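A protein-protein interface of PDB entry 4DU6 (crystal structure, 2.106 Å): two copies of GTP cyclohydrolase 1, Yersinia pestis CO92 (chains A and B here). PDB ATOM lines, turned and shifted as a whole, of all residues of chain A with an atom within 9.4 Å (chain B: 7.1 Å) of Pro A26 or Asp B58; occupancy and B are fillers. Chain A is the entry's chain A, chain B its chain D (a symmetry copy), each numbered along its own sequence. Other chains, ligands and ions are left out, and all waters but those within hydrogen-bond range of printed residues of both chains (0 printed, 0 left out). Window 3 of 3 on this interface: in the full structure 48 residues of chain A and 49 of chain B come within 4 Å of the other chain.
N of Asp B55 is in hydrogen-bond range of O of Pro A26, 2.9 Å away. The backbone carbonyl oxygen (O) of Asn B53 is in hydrogen-bond range of the backbone NH (N) of Arg A28, at 2.8 Å. The guanidinium group (NE) of Arg A28 lies within salt-bridge range of the side-chain carboxylate (OD1) of Asp B55, at 3.4 Å. A ring nitrogen (NE2) of His A114 lies within hydrogen-bond range of the side-chain hydroxyl (OG) of Ser B60. The side-chain carboxylate (OE2) of Glu A113 lies close to the side-chain hydroxyl (OG) of Ser B60 (2.4 Å).
The backbone NH (N) of Glu A113 lies within hydrogen-bond range of the backbone carbonyl oxygen (O) of Gln A151, 2.9 Å away. NH1 of Arg A155 lies within salt-bridge range of OE1 of Glu A113, 2.6 Å away. OD1 of Asp B55 sits at hydrogen-bond distance from OG1 of Thr B57, at 2.7 Å. The backbone NH (N) of Ser B60 sits at hydrogen-bond distance from the side-chain carboxylate (OD2) of Asp B58, at 2.7 Å. The side-chain carboxylate (OD2) of Asp B58 is in hydrogen-bond range of the backbone NH (N) of Leu B61, at 3.4 Å.
Pro A26 touches Leu B54. CG of Pro A26 touches OD1 of Asp B58 (3.2 Å). Pro A26 touches Leu B61 (CB to CD1, 3.98 Å). CA of Leu A27 touches O of Asn B53, at 3.3 Å. Asp B55 touches Leu A27. CG2 of Thr B57 touches NH1 of Arg A28, at 3.96 Å. Leu A80 touches Leu B52. CB of Glu A113 touches CD2 of Leu B61 (3.6 Å). Leu B54 touches Pro A150 (CD1 to CG, 3.8 Å). Val A152 touches Ser B60.
Of the printed residues of chain B, Pro A26 touches Leu B54, Asp B55, Asp B58 and Leu B61. Of the printed residues of chain B, Leu A27 touches Asn B53 and Asp B55. Of the printed residues of chain B, Arg A28 touches Asn B53, Asp B55 and Thr B57. Gln A151 touches none of the printed residues of chain B. Of the printed residues of chain A, Leu B52 touches Leu A80. Printed residues of chain A within 4 Å of Asp B55: Pro A26 (2.9 Å), Leu A27 (3.9 Å) and Arg A28 (3.4 Å). Of chain A, only Pro A26 (3.2 Å) comes within 4 Å of Asp B58. Of chain A, only Glu A113 (2.4 Å), His A114 (2.8 Å) and Val A152 (3.8 Å) come within 4 Å of Ser B60. Of the printed residues of chain A, Leu B61 touches Pro A26 (3.98 Å) and Glu A113 (3.6 Å). The nearest printed residue of chain B that does not touch Pro A26 is Asn B53 (4.1 Å). The nearest printed residue of chain A that does not touch Leu B54 is Arg A28 (4.02 Å).
Hydrophobic or aromatic side chains of chain B within 4 Å of the printed part of chain A: Leu B54 and Leu B61. Among the printed residues, 15 pairs touch across the chains.
No position is printed for both chains. Of the 15 pairs that touch across the chains among the printed residues, none has its exchanged pair printed and touching as well.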
ATOM      1  N   HIS A  15      13.575  -3.165   6.623  1.00  0.00           N
ATOM      2  CA  HIS A  15      13.586  -2.412   7.880  1.00  0.00           C
ATOM      3  C   HIS A  15      14.690  -1.361   7.885  1.00  0.00           C
ATOM      4  O   HIS A  15      14.470  -0.227   8.306  1.00  0.00           O
ATOM      5  CB  HIS A  15      13.688  -3.371   9.085  1.00  0.00           C
ATOM      6  CG  HIS A  15      13.988  -2.707  10.404  1.00  0.00           C
ATOM      7  ND1 HIS A  15      13.212  -1.702  10.940  1.00  0.00           N
ATOM      8  CD2 HIS A  15      14.953  -2.963  11.322  1.00  0.00           C
ATOM      9  CE1 HIS A  15      13.701  -1.344  12.114  1.00  0.00           C
ATOM     10  NE2 HIS A  15      14.760  -2.088  12.365  1.00  0.00           N
ATOM     11  N   LEU A  18      13.800   1.527   5.396  1.00  0.00           N
ATOM     12  CA  LEU A  18      12.834   2.430   6.012  1.00  0.00           C
ATOM     13  C   LEU A  18      13.482   3.311   7.069  1.00  0.00           C
ATOM     14  O   LEU A  18      13.164   4.496   7.161  1.00  0.00           O
ATOM     15  CB  LEU A  18      11.634   1.669   6.583  1.00  0.00           C
ATOM     16  CG  LEU A  18      10.418   1.557   5.618  1.00  0.00           C
ATOM     17  CD1 LEU A  18      10.781   0.744   4.422  1.00  0.00           C
ATOM     18  CD2 LEU A  18       9.225   0.953   6.316  1.00  0.00           C
ATOM     19  N   LEU A  19      14.398   2.744   7.860  1.00  0.00           N
ATOM     20  CA  LEU A  19      15.085   3.539   8.892  1.00  0.00           C
ATOM     21  C   LEU A  19      16.014   4.578   8.298  1.00  0.00           C
ATOM     22  O   LEU A  19      16.107   5.680   8.810  1.00  0.00           O
ATOM     23  CB  LEU A  19      15.889   2.656   9.868  1.00  0.00           C
ATOM     24  CG  LEU A  19      15.188   2.085  11.098  1.00  0.00           C
ATOM     25  CD1 LEU A  19      16.125   1.052  11.727  1.00  0.00           C
ATOM     26  CD2 LEU A  19      14.796   3.189  12.110  1.00  0.00           C
ATOM     27  N   GLY A  22      13.929   7.481   7.003  1.00  0.00           N
ATOM     28  CA  GLY A  22      13.289   8.258   8.061  1.00  0.00           C
ATOM     29  C   GLY A  22      11.820   7.888   8.169  1.00  0.00           C
ATOM     30  O   GLY A  22      10.995   8.626   8.684  1.00  0.00           O
ATOM     31  N   LEU A  23      11.502   6.705   7.667  1.00  0.00           N
ATOM     32  CA  LEU A  23      10.132   6.346   7.382  1.00  0.00           C
ATOM     33  C   LEU A  23       9.587   5.266   8.291  1.00  0.00           C
ATOM     34  O   LEU A  23       8.418   4.919   8.201  1.00  0.00           O
ATOM     35  CB  LEU A  23      10.055   5.871   5.928  1.00  0.00           C
ATOM     36  CG  LEU A  23       8.747   5.796   5.153  1.00  0.00           C
ATOM     37  CD1 LEU A  23       7.987   7.079   5.275  1.00  0.00           C
ATOM     38  CD2 LEU A  23       9.069   5.457   3.673  1.00  0.00           C
ATOM     39  N   GLU A  24      10.416   4.706   9.164  1.00  0.00           N
ATOM     40  CA  GLU A  24       9.919   3.602   9.970  1.00  0.00           C
ATOM     41  C   GLU A  24       8.827   4.108  10.935  1.00  0.00           C
ATOM     42  O   GLU A  24       8.835   5.267  11.350  1.00  0.00           O
ATOM     43  CB  GLU A  24      11.070   2.860  10.665  1.00  0.00           C
ATOM     44  CG  GLU A  24      10.702   1.513  11.298  1.00  0.00           C
ATOM     45  CD  GLU A  24      10.109   0.521  10.289  1.00  0.00           C
ATOM     46  OE1 GLU A  24       8.874   0.511  10.118  1.00  0.00           O
ATOM     47  OE2 GLU A  24      10.869  -0.253   9.675  1.00  0.00           O
ATOM     48  N   THR A  25       7.854   3.249  11.229  1.00  0.00           N
ATOM     49  CA  THR A  25       6.886   3.492  12.298  1.00  0.00           C
ATOM     50  C   THR A  25       7.675   3.693  13.603  1.00  0.00           C
ATOM     51  O   THR A  25       8.593   2.910  13.876  1.00  0.00           O
ATOM     52  CB  THR A  25       5.936   2.267  12.432  1.00  0.00           C
ATOM     53  OG1 THR A  25       5.047   2.230  11.301  1.00  0.00           O
ATOM     54  CG2 THR A  25       5.122   2.323  13.714  1.00  0.00           C
ATOM     55  N   PRO A  26       7.350   4.758  14.376  1.00  0.00           N
ATOM     56  CA  PRO A  26       8.050   5.097  15.643  1.00  0.00           C
ATOM     57  C   PRO A  26       8.020   3.943  16.656  1.00  0.00           C
ATOM     58  O   PRO A  26       7.003   3.734  17.319  1.00  0.00           O
ATOM     59  CB  PRO A  26       7.280   6.317  16.168  1.00  0.00           C
ATOM     60  CG  PRO A  26       6.718   6.948  14.924  1.00  0.00           C
ATOM     61  CD  PRO A  26       6.409   5.817  13.965  1.00  0.00           C
ATOM     62  N   LEU A  27       9.120   3.191  16.720  1.00  0.00           N
ATOM     63  CA  LEU A  27       9.209   1.997  17.549  1.00  0.00           C
ATOM     64  C   LEU A  27      10.327   2.143  18.594  1.00  0.00           C
ATOM     65  O   LEU A  27      11.303   2.864  18.367  1.00  0.00           O
ATOM     66  CB  LEU A  27       9.473   0.767  16.695  1.00  0.00           C
ATOM     67  CG  LEU A  27       8.292   0.310  15.812  1.00  0.00           C
ATOM     68  CD1 LEU A  27       8.613  -0.966  15.006  1.00  0.00           C
ATOM     69  CD2 LEU A  27       7.054   0.126  16.686  1.00  0.00           C
ATOM     70  N   ARG A  28      10.165   1.478  19.737  1.00  0.00           N
ATOM     71  CA  ARG A  28      11.250   1.314  20.722  1.00  0.00           C
ATOM     72  C   ARG A  28      11.660  -0.149  20.769  1.00  0.00           C
ATOM     73  O   ARG A  28      11.035  -0.994  20.134  1.00  0.00           O
ATOM     74  CB  ARG A  28      10.798   1.729  22.119  1.00  0.00           C
ATOM     75  CG  ARG A  28      10.374   3.161  22.227  1.00  0.00           C
ATOM     76  CD  ARG A  28      11.393   3.998  22.997  1.00  0.00           C
ATOM     77  NE  ARG A  28      10.826   5.298  23.354  1.00  0.00           N
ATOM     78  CZ  ARG A  28       9.909   5.473  24.303  1.00  0.00           C
ATOM     79  NH1 ARG A  28       9.440   6.690  24.552  1.00  0.00           N
ATOM     80  NH2 ARG A  28       9.456   4.429  24.999  1.00  0.00           N
ATOM     81  N   LYS A  29      12.688  -0.465  21.544  1.00  0.00           N
ATOM     82  CA  LYS A  29      13.089  -1.863  21.687  1.00  0.00           C
ATOM     83  C   LYS A  29      12.334  -2.569  22.816  1.00  0.00           C
ATOM     84  O   LYS A  29      12.198  -2.029  23.898  1.00  0.00           O
ATOM     85  CB  LYS A  29      14.612  -1.985  21.833  1.00  0.00           C
ATOM     86  CG  LYS A  29      15.354  -1.661  20.512  1.00  0.00           C
ATOM     87  CD  LYS A  29      14.560  -2.089  19.240  1.00  0.00           C
ATOM     88  CE  LYS A  29      15.380  -1.858  17.970  1.00  0.00           C
ATOM     89  NZ  LYS A  29      14.589  -1.969  16.688  1.00  0.00           N
ATOM     90  N   LEU A  80       4.173  -4.728  13.444  1.00  0.00           N
ATOM     91  CA  LEU A  80       5.173  -4.011  14.239  1.00  0.00           C
ATOM     92  C   LEU A  80       6.356  -4.940  14.490  1.00  0.00           C
ATOM     93  O   LEU A  80       7.383  -4.511  14.971  1.00  0.00           O
ATOM     94  CB  LEU A  80       4.605  -3.539  15.596  1.00  0.00           C
ATOM     95  CG  LEU A  80       3.498  -2.470  15.583  1.00  0.00           C
ATOM     96  CD1 LEU A  80       3.006  -2.156  16.984  1.00  0.00           C
ATOM     97  CD2 LEU A  80       3.992  -1.213  14.925  1.00  0.00           C
ATOM     98  N   GLU A 113      -3.600   5.917  13.788  1.00  0.00           N
ATOM     99  CA  GLU A 113      -2.736   6.016  14.936  1.00  0.00           C
ATOM    100  C   GLU A 113      -3.174   7.121  15.881  1.00  0.00           C
ATOM    101  O   GLU A 113      -2.697   7.185  17.026  1.00  0.00           O
ATOM    102  CB  GLU A 113      -1.282   6.164  14.537  1.00  0.00           C
ATOM    103  CG  GLU A 113      -0.903   7.524  14.099  1.00  0.00           C
ATOM    104  CD  GLU A 113       0.524   7.550  13.591  1.00  0.00           C
ATOM    105  OE1 GLU A 113       0.967   6.528  13.034  1.00  0.00           O
ATOM    106  OE2 GLU A 113       1.203   8.581  13.750  1.00  0.00           O
ATOM    107  N   HIS A 114      -4.092   7.968  15.428  1.00  0.00           N
ATOM    108  CA  HIS A 114      -4.513   9.123  16.242  1.00  0.00           C
ATOM    109  C   HIS A 114      -5.644   8.778  17.169  1.00  0.00           C
ATOM    110  O   HIS A 114      -5.782   9.387  18.239  1.00  0.00           O
ATOM    111  CB  HIS A 114      -4.970  10.279  15.353  1.00  0.00           C
ATOM    112  CG  HIS A 114      -3.844  10.987  14.681  1.00  0.00           C
ATOM    113  ND1 HIS A 114      -4.038  11.953  13.719  1.00  0.00           N
ATOM    114  CD2 HIS A 114      -2.504  10.859  14.825  1.00  0.00           C
ATOM    115  CE1 HIS A 114      -2.865  12.401  13.307  1.00  0.00           C
ATOM    116  NE2 HIS A 114      -1.918  11.749  13.957  1.00  0.00           N
ATOM    117  N   ARG A 149      -0.394  -2.036  11.522  1.00  0.00           N
ATOM    118  CA  ARG A 149       0.290  -1.126  12.422  1.00  0.00           C
ATOM    119  C   ARG A 149      -0.693   0.009  12.710  1.00  0.00           C
ATOM    120  O   ARG A 149      -1.626   0.195  11.971  1.00  0.00           O
ATOM    121  CB  ARG A 149       1.538  -0.560  11.751  1.00  0.00           C
ATOM    122  CG  ARG A 149       2.592  -1.574  11.387  1.00  0.00           C
ATOM    123  CD  ARG A 149       3.714  -0.968  10.586  1.00  0.00           C
ATOM    124  NE  ARG A 149       4.839  -1.888  10.537  1.00  0.00           N
ATOM    125  CZ  ARG A 149       6.071  -1.535  10.202  1.00  0.00           C
ATOM    126  NH1 ARG A 149       6.327  -0.281   9.858  1.00  0.00           N
ATOM    127  NH2 ARG A 149       7.051  -2.429  10.220  1.00  0.00           N
ATOM    128  N   PRO A 150      -0.497   0.752  13.813  1.00  0.00           N
ATOM    129  CA  PRO A 150      -1.157   2.052  13.903  1.00  0.00           C
ATOM    130  C   PRO A 150      -0.548   2.856  12.775  1.00  0.00           C
ATOM    131  O   PRO A 150       0.672   2.842  12.598  1.00  0.00           O
ATOM    132  CB  PRO A 150      -0.695   2.620  15.279  1.00  0.00           C
ATOM    133  CG  PRO A 150      -0.001   1.476  15.996  1.00  0.00           C
ATOM    134  CD  PRO A 150       0.449   0.507  14.913  1.00  0.00           C
ATOM    135  N   GLN A 151      -1.370   3.531  11.994  1.00  0.00           N
ATOM    136  CA  GLN A 151      -0.862   4.183  10.797  1.00  0.00           C
ATOM    137  C   GLN A 151      -1.467   5.566  10.568  1.00  0.00           C
ATOM    138  O   GLN A 151      -2.553   5.908  11.042  1.00  0.00           O
ATOM    139  CB  GLN A 151      -1.153   3.314   9.523  1.00  0.00           C
ATOM    140  CG  GLN A 151      -0.191   2.136   9.329  1.00  0.00           C
ATOM    141  CD  GLN A 151       1.200   2.578   8.931  1.00  0.00           C
ATOM    142  OE1 GLN A 151       1.497   3.765   8.866  1.00  0.00           O
ATOM    143  NE2 GLN A 151       2.057   1.626   8.663  1.00  0.00           N
ATOM    144  N   VAL A 152      -0.714   6.338   9.816  1.00  0.00           N
ATOM    145  CA  VAL A 152      -1.200   7.481   9.097  1.00  0.00           C
ATOM    146  C   VAL A 152      -1.165   7.026   7.621  1.00  0.00           C
ATOM    147  O   VAL A 152      -0.173   6.427   7.188  1.00  0.00           O
ATOM    148  CB  VAL A 152      -0.270   8.643   9.388  1.00  0.00           C
ATOM    149  CG1 VAL A 152      -0.460   9.748   8.415  1.00  0.00           C
ATOM    150  CG2 VAL A 152      -0.531   9.118  10.816  1.00  0.00           C
ATOM    151  N   ARG A 155       1.726   7.758   5.425  1.00  0.00           N
ATOM    152  CA  ARG A 155       2.948   7.013   5.795  1.00  0.00           C
ATOM    153  C   ARG A 155       2.906   5.569   5.293  1.00  0.00           C
ATOM    154  O   ARG A 155       3.905   5.052   4.786  1.00  0.00           O
ATOM    155  CB  ARG A 155       3.178   6.968   7.307  1.00  0.00           C
ATOM    156  CG  ARG A 155       4.558   6.441   7.670  1.00  0.00           C
ATOM    157  CD  ARG A 155       4.725   6.141   9.158  1.00  0.00           C
ATOM    158  NE  ARG A 155       4.500   7.307  10.024  1.00  0.00           N
ATOM    159  CZ  ARG A 155       3.531   7.369  10.930  1.00  0.00           C
ATOM    160  NH1 ARG A 155       2.701   6.343  11.073  1.00  0.00           N
ATOM    161  NH2 ARG A 155       3.371   8.443  11.670  1.00  0.00           N
ATOM    162  N   GLN A 159       5.609   3.544   2.863  1.00  0.00           N
ATOM    163  CA  GLN A 159       6.389   2.454   3.446  1.00  0.00           C
ATOM    164  C   GLN A 159       6.225   1.264   2.504  1.00  0.00           C
ATOM    165  O   GLN A 159       7.193   0.544   2.228  1.00  0.00           O
ATOM    166  CB  GLN A 159       5.914   2.057   4.864  1.00  0.00           C
ATOM    167  CG  GLN A 159       6.090   3.081   5.957  1.00  0.00           C
ATOM    168  CD  GLN A 159       5.561   2.606   7.302  1.00  0.00           C
ATOM    169  OE1 GLN A 159       4.562   1.895   7.375  1.00  0.00           O
ATOM    170  NE2 GLN A 159       6.225   3.020   8.383  1.00  0.00           N
ATOM    171  N   LEU B  52       3.149  -1.779  23.472  1.00  0.00           N
ATOM    172  CA  LEU B  52       3.113  -2.228  22.080  1.00  0.00           C
ATOM    173  C   LEU B  52       4.445  -1.922  21.381  1.00  0.00           C
ATOM    174  O   LEU B  52       4.596  -2.232  20.198  1.00  0.00           O
ATOM    175  CB  LEU B  52       1.933  -1.604  21.356  1.00  0.00           C
ATOM    176  CG  LEU B  52       0.611  -2.287  21.694  1.00  0.00           C
ATOM    177  CD1 LEU B  52      -0.619  -1.433  21.259  1.00  0.00           C
ATOM    178  CD2 LEU B  52       0.557  -3.679  21.021  1.00  0.00           C
ATOM    179  N   ASN B  53       5.389  -1.336  22.140  1.00  0.00           N
ATOM    180  CA  ASN B  53       6.690  -0.880  21.644  1.00  0.00           C
ATOM    181  C   ASN B  53       6.608   0.394  20.806  1.00  0.00           C
ATOM    182  O   ASN B  53       7.517   0.695  20.036  1.00  0.00           O
ATOM    183  CB  ASN B  53       7.447  -1.965  20.848  1.00  0.00           C
ATOM    184  CG  ASN B  53       7.588  -3.274  21.614  1.00  0.00           C
ATOM    185  OD1 ASN B  53       7.294  -4.349  21.098  1.00  0.00           O
ATOM    186  ND2 ASN B  53       8.018  -3.182  22.849  1.00  0.00           N
ATOM    187  N   LEU B  54       5.533   1.150  20.956  1.00  0.00           N
ATOM    188  CA  LEU B  54       5.407   2.377  20.204  1.00  0.00           C
ATOM    189  C   LEU B  54       6.179   3.486  20.879  1.00  0.00           C
ATOM    190  O   LEU B  54       6.370   3.472  22.087  1.00  0.00           O
ATOM    191  CB  LEU B  54       3.932   2.748  20.008  1.00  0.00           C
ATOM    192  CG  LEU B  54       3.184   1.741  19.123  1.00  0.00           C
ATOM    193  CD1 LEU B  54       1.683   1.891  19.329  1.00  0.00           C
ATOM    194  CD2 LEU B  54       3.553   1.959  17.650  1.00  0.00           C
ATOM    195  N   ASP B  55       6.633   4.446  20.087  1.00  0.00           N
ATOM    196  CA  ASP B  55       7.487   5.518  20.588  1.00  0.00           C
ATOM    197  C   ASP B  55       6.706   6.821  20.792  1.00  0.00           C
ATOM    198  O   ASP B  55       6.511   7.577  19.844  1.00  0.00           O
ATOM    199  CB  ASP B  55       8.638   5.741  19.599  1.00  0.00           C
ATOM    200  CG  ASP B  55       9.694   6.715  20.118  1.00  0.00           C
ATOM    201  OD1 ASP B  55       9.445   7.412  21.129  1.00  0.00           O
ATOM    202  OD2 ASP B  55      10.773   6.797  19.489  1.00  0.00           O
ATOM    203  N   LEU B  56       6.333   7.111  22.040  1.00  0.00           N
ATOM    204  CA  LEU B  56       5.478   8.253  22.335  1.00  0.00           C
ATOM    205  C   LEU B  56       6.152   9.607  22.198  1.00  0.00           C
ATOM    206  O   LEU B  56       5.510  10.644  22.385  1.00  0.00           O
ATOM    207  CB  LEU B  56       4.864   8.137  23.724  1.00  0.00           C
ATOM    208  CG  LEU B  56       4.009   6.893  23.941  1.00  0.00           C
ATOM    209  CD1 LEU B  56       3.510   6.844  25.369  1.00  0.00           C
ATOM    210  CD2 LEU B  56       2.856   6.908  22.985  1.00  0.00           C
ATOM    211  N   THR B  57       7.438   9.628  21.875  1.00  0.00           N
ATOM    212  CA  THR B  57       8.068  10.923  21.635  1.00  0.00           C
ATOM    213  C   THR B  57       7.715  11.440  20.247  1.00  0.00           C
ATOM    214  O   THR B  57       7.962  12.608  19.921  1.00  0.00           O
ATOM    215  CB  THR B  57       9.581  10.892  21.828  1.00  0.00           C
ATOM    216  OG1 THR B  57      10.167  10.021  20.863  1.00  0.00           O
ATOM    217  CG2 THR B  57       9.919  10.396  23.229  1.00  0.00           C
ATOM    218  N   ASP B  58       7.115  10.573  19.431  1.00  0.00           N
ATOM    219  CA  ASP B  58       6.664  10.987  18.113  1.00  0.00           C
ATOM    220  C   ASP B  58       5.495  11.971  18.222  1.00  0.00           C
ATOM    221  O   ASP B  58       4.524  11.704  18.932  1.00  0.00           O
ATOM    222  CB  ASP B  58       6.247   9.783  17.268  1.00  0.00           C
ATOM    223  CG  ASP B  58       5.914  10.186  15.846  1.00  0.00           C
ATOM    224  OD1 ASP B  58       6.844  10.166  15.019  1.00  0.00           O
ATOM    225  OD2 ASP B  58       4.756  10.580  15.574  1.00  0.00           O
ATOM    226  N   ASP B  59       5.591  13.099  17.517  1.00  0.00           N
ATOM    227  CA  ASP B  59       4.530  14.108  17.536  1.00  0.00           C
ATOM    228  C   ASP B  59       3.159  13.525  17.165  1.00  0.00           C
ATOM    229  O   ASP B  59       2.129  13.869  17.749  1.00  0.00           O
ATOM    230  CB  ASP B  59       4.874  15.286  16.602  1.00  0.00           C
ATOM    231  CG  ASP B  59       4.729  14.932  15.111  1.00  0.00           C
ATOM    232  OD1 ASP B  59       5.112  13.803  14.726  1.00  0.00           O
ATOM    233  OD2 ASP B  59       4.236  15.787  14.336  1.00  0.00           O
ATOM    234  N   SER B  60       3.142  12.629  16.193  1.00  0.00           N
ATOM    235  CA  SER B  60       1.872  12.092  15.739  1.00  0.00           C
ATOM    236  C   SER B  60       1.207  11.138  16.746  1.00  0.00           C
ATOM    237  O   SER B  60      -0.028  11.087  16.816  1.00  0.00           O
ATOM    238  CB  SER B  60       1.999  11.465  14.340  1.00  0.00           C
ATOM    239  OG  SER B  60       0.776  10.898  13.907  1.00  0.00           O
ATOM    240  N   LEU B  61       2.004  10.393  17.512  1.00  0.00           N
ATOM    241  CA  LEU B  61       1.471   9.462  18.510  1.00  0.00           C
ATOM    242  C   LEU B  61       1.284  10.090  19.915  1.00  0.00           C
ATOM    243  O   LEU B  61       0.522   9.585  20.731  1.00  0.00           O
ATOM    244  CB  LEU B  61       2.421   8.266  18.681  1.00  0.00           C
ATOM    245  CG  LEU B  61       2.572   7.365  17.468  1.00  0.00           C
ATOM    246  CD1 LEU B  61       3.613   6.268  17.718  1.00  0.00           C
ATOM    247  CD2 LEU B  61       1.214   6.768  17.097  1.00  0.00           C
ATOM    248  N   ALA B  62       1.982  11.180  20.178  1.00  0.00           N
ATOM    249  CA  ALA B  62       2.068  11.729  21.537  1.00  0.00           C
ATOM    250  C   ALA B  62       0.703  11.970  22.187  1.00  0.00           C
ATOM    251  O   ALA B  62       0.486  11.692  23.367  1.00  0.00           O
ATOM    252  CB  ALA B  62       2.880  13.007  21.532  1.00  0.00           C
ATOM    253  N   ASP B  63      -0.237  12.456  21.400  1.00  0.00           N
ATOM    254  CA  ASP B  63      -1.516  12.838  21.964  1.00  0.00           C
ATOM    255  C   ASP B  63      -2.548  11.720  21.878  1.00  0.00           C
ATOM    256  O   ASP B  63      -3.676  11.889  22.315  1.00  0.00           O
ATOM    257  CB  ASP B  63      -2.009  14.144  21.335  1.00  0.00           C
ATOM    258  CG  ASP B  63      -0.942  15.255  21.381  1.00  0.00           C
ATOM    259  OD1 ASP B  63      -0.809  15.940  22.426  1.00  0.00           O
ATOM    260  OD2 ASP B  63      -0.224  15.426  20.367  1.00  0.00           O
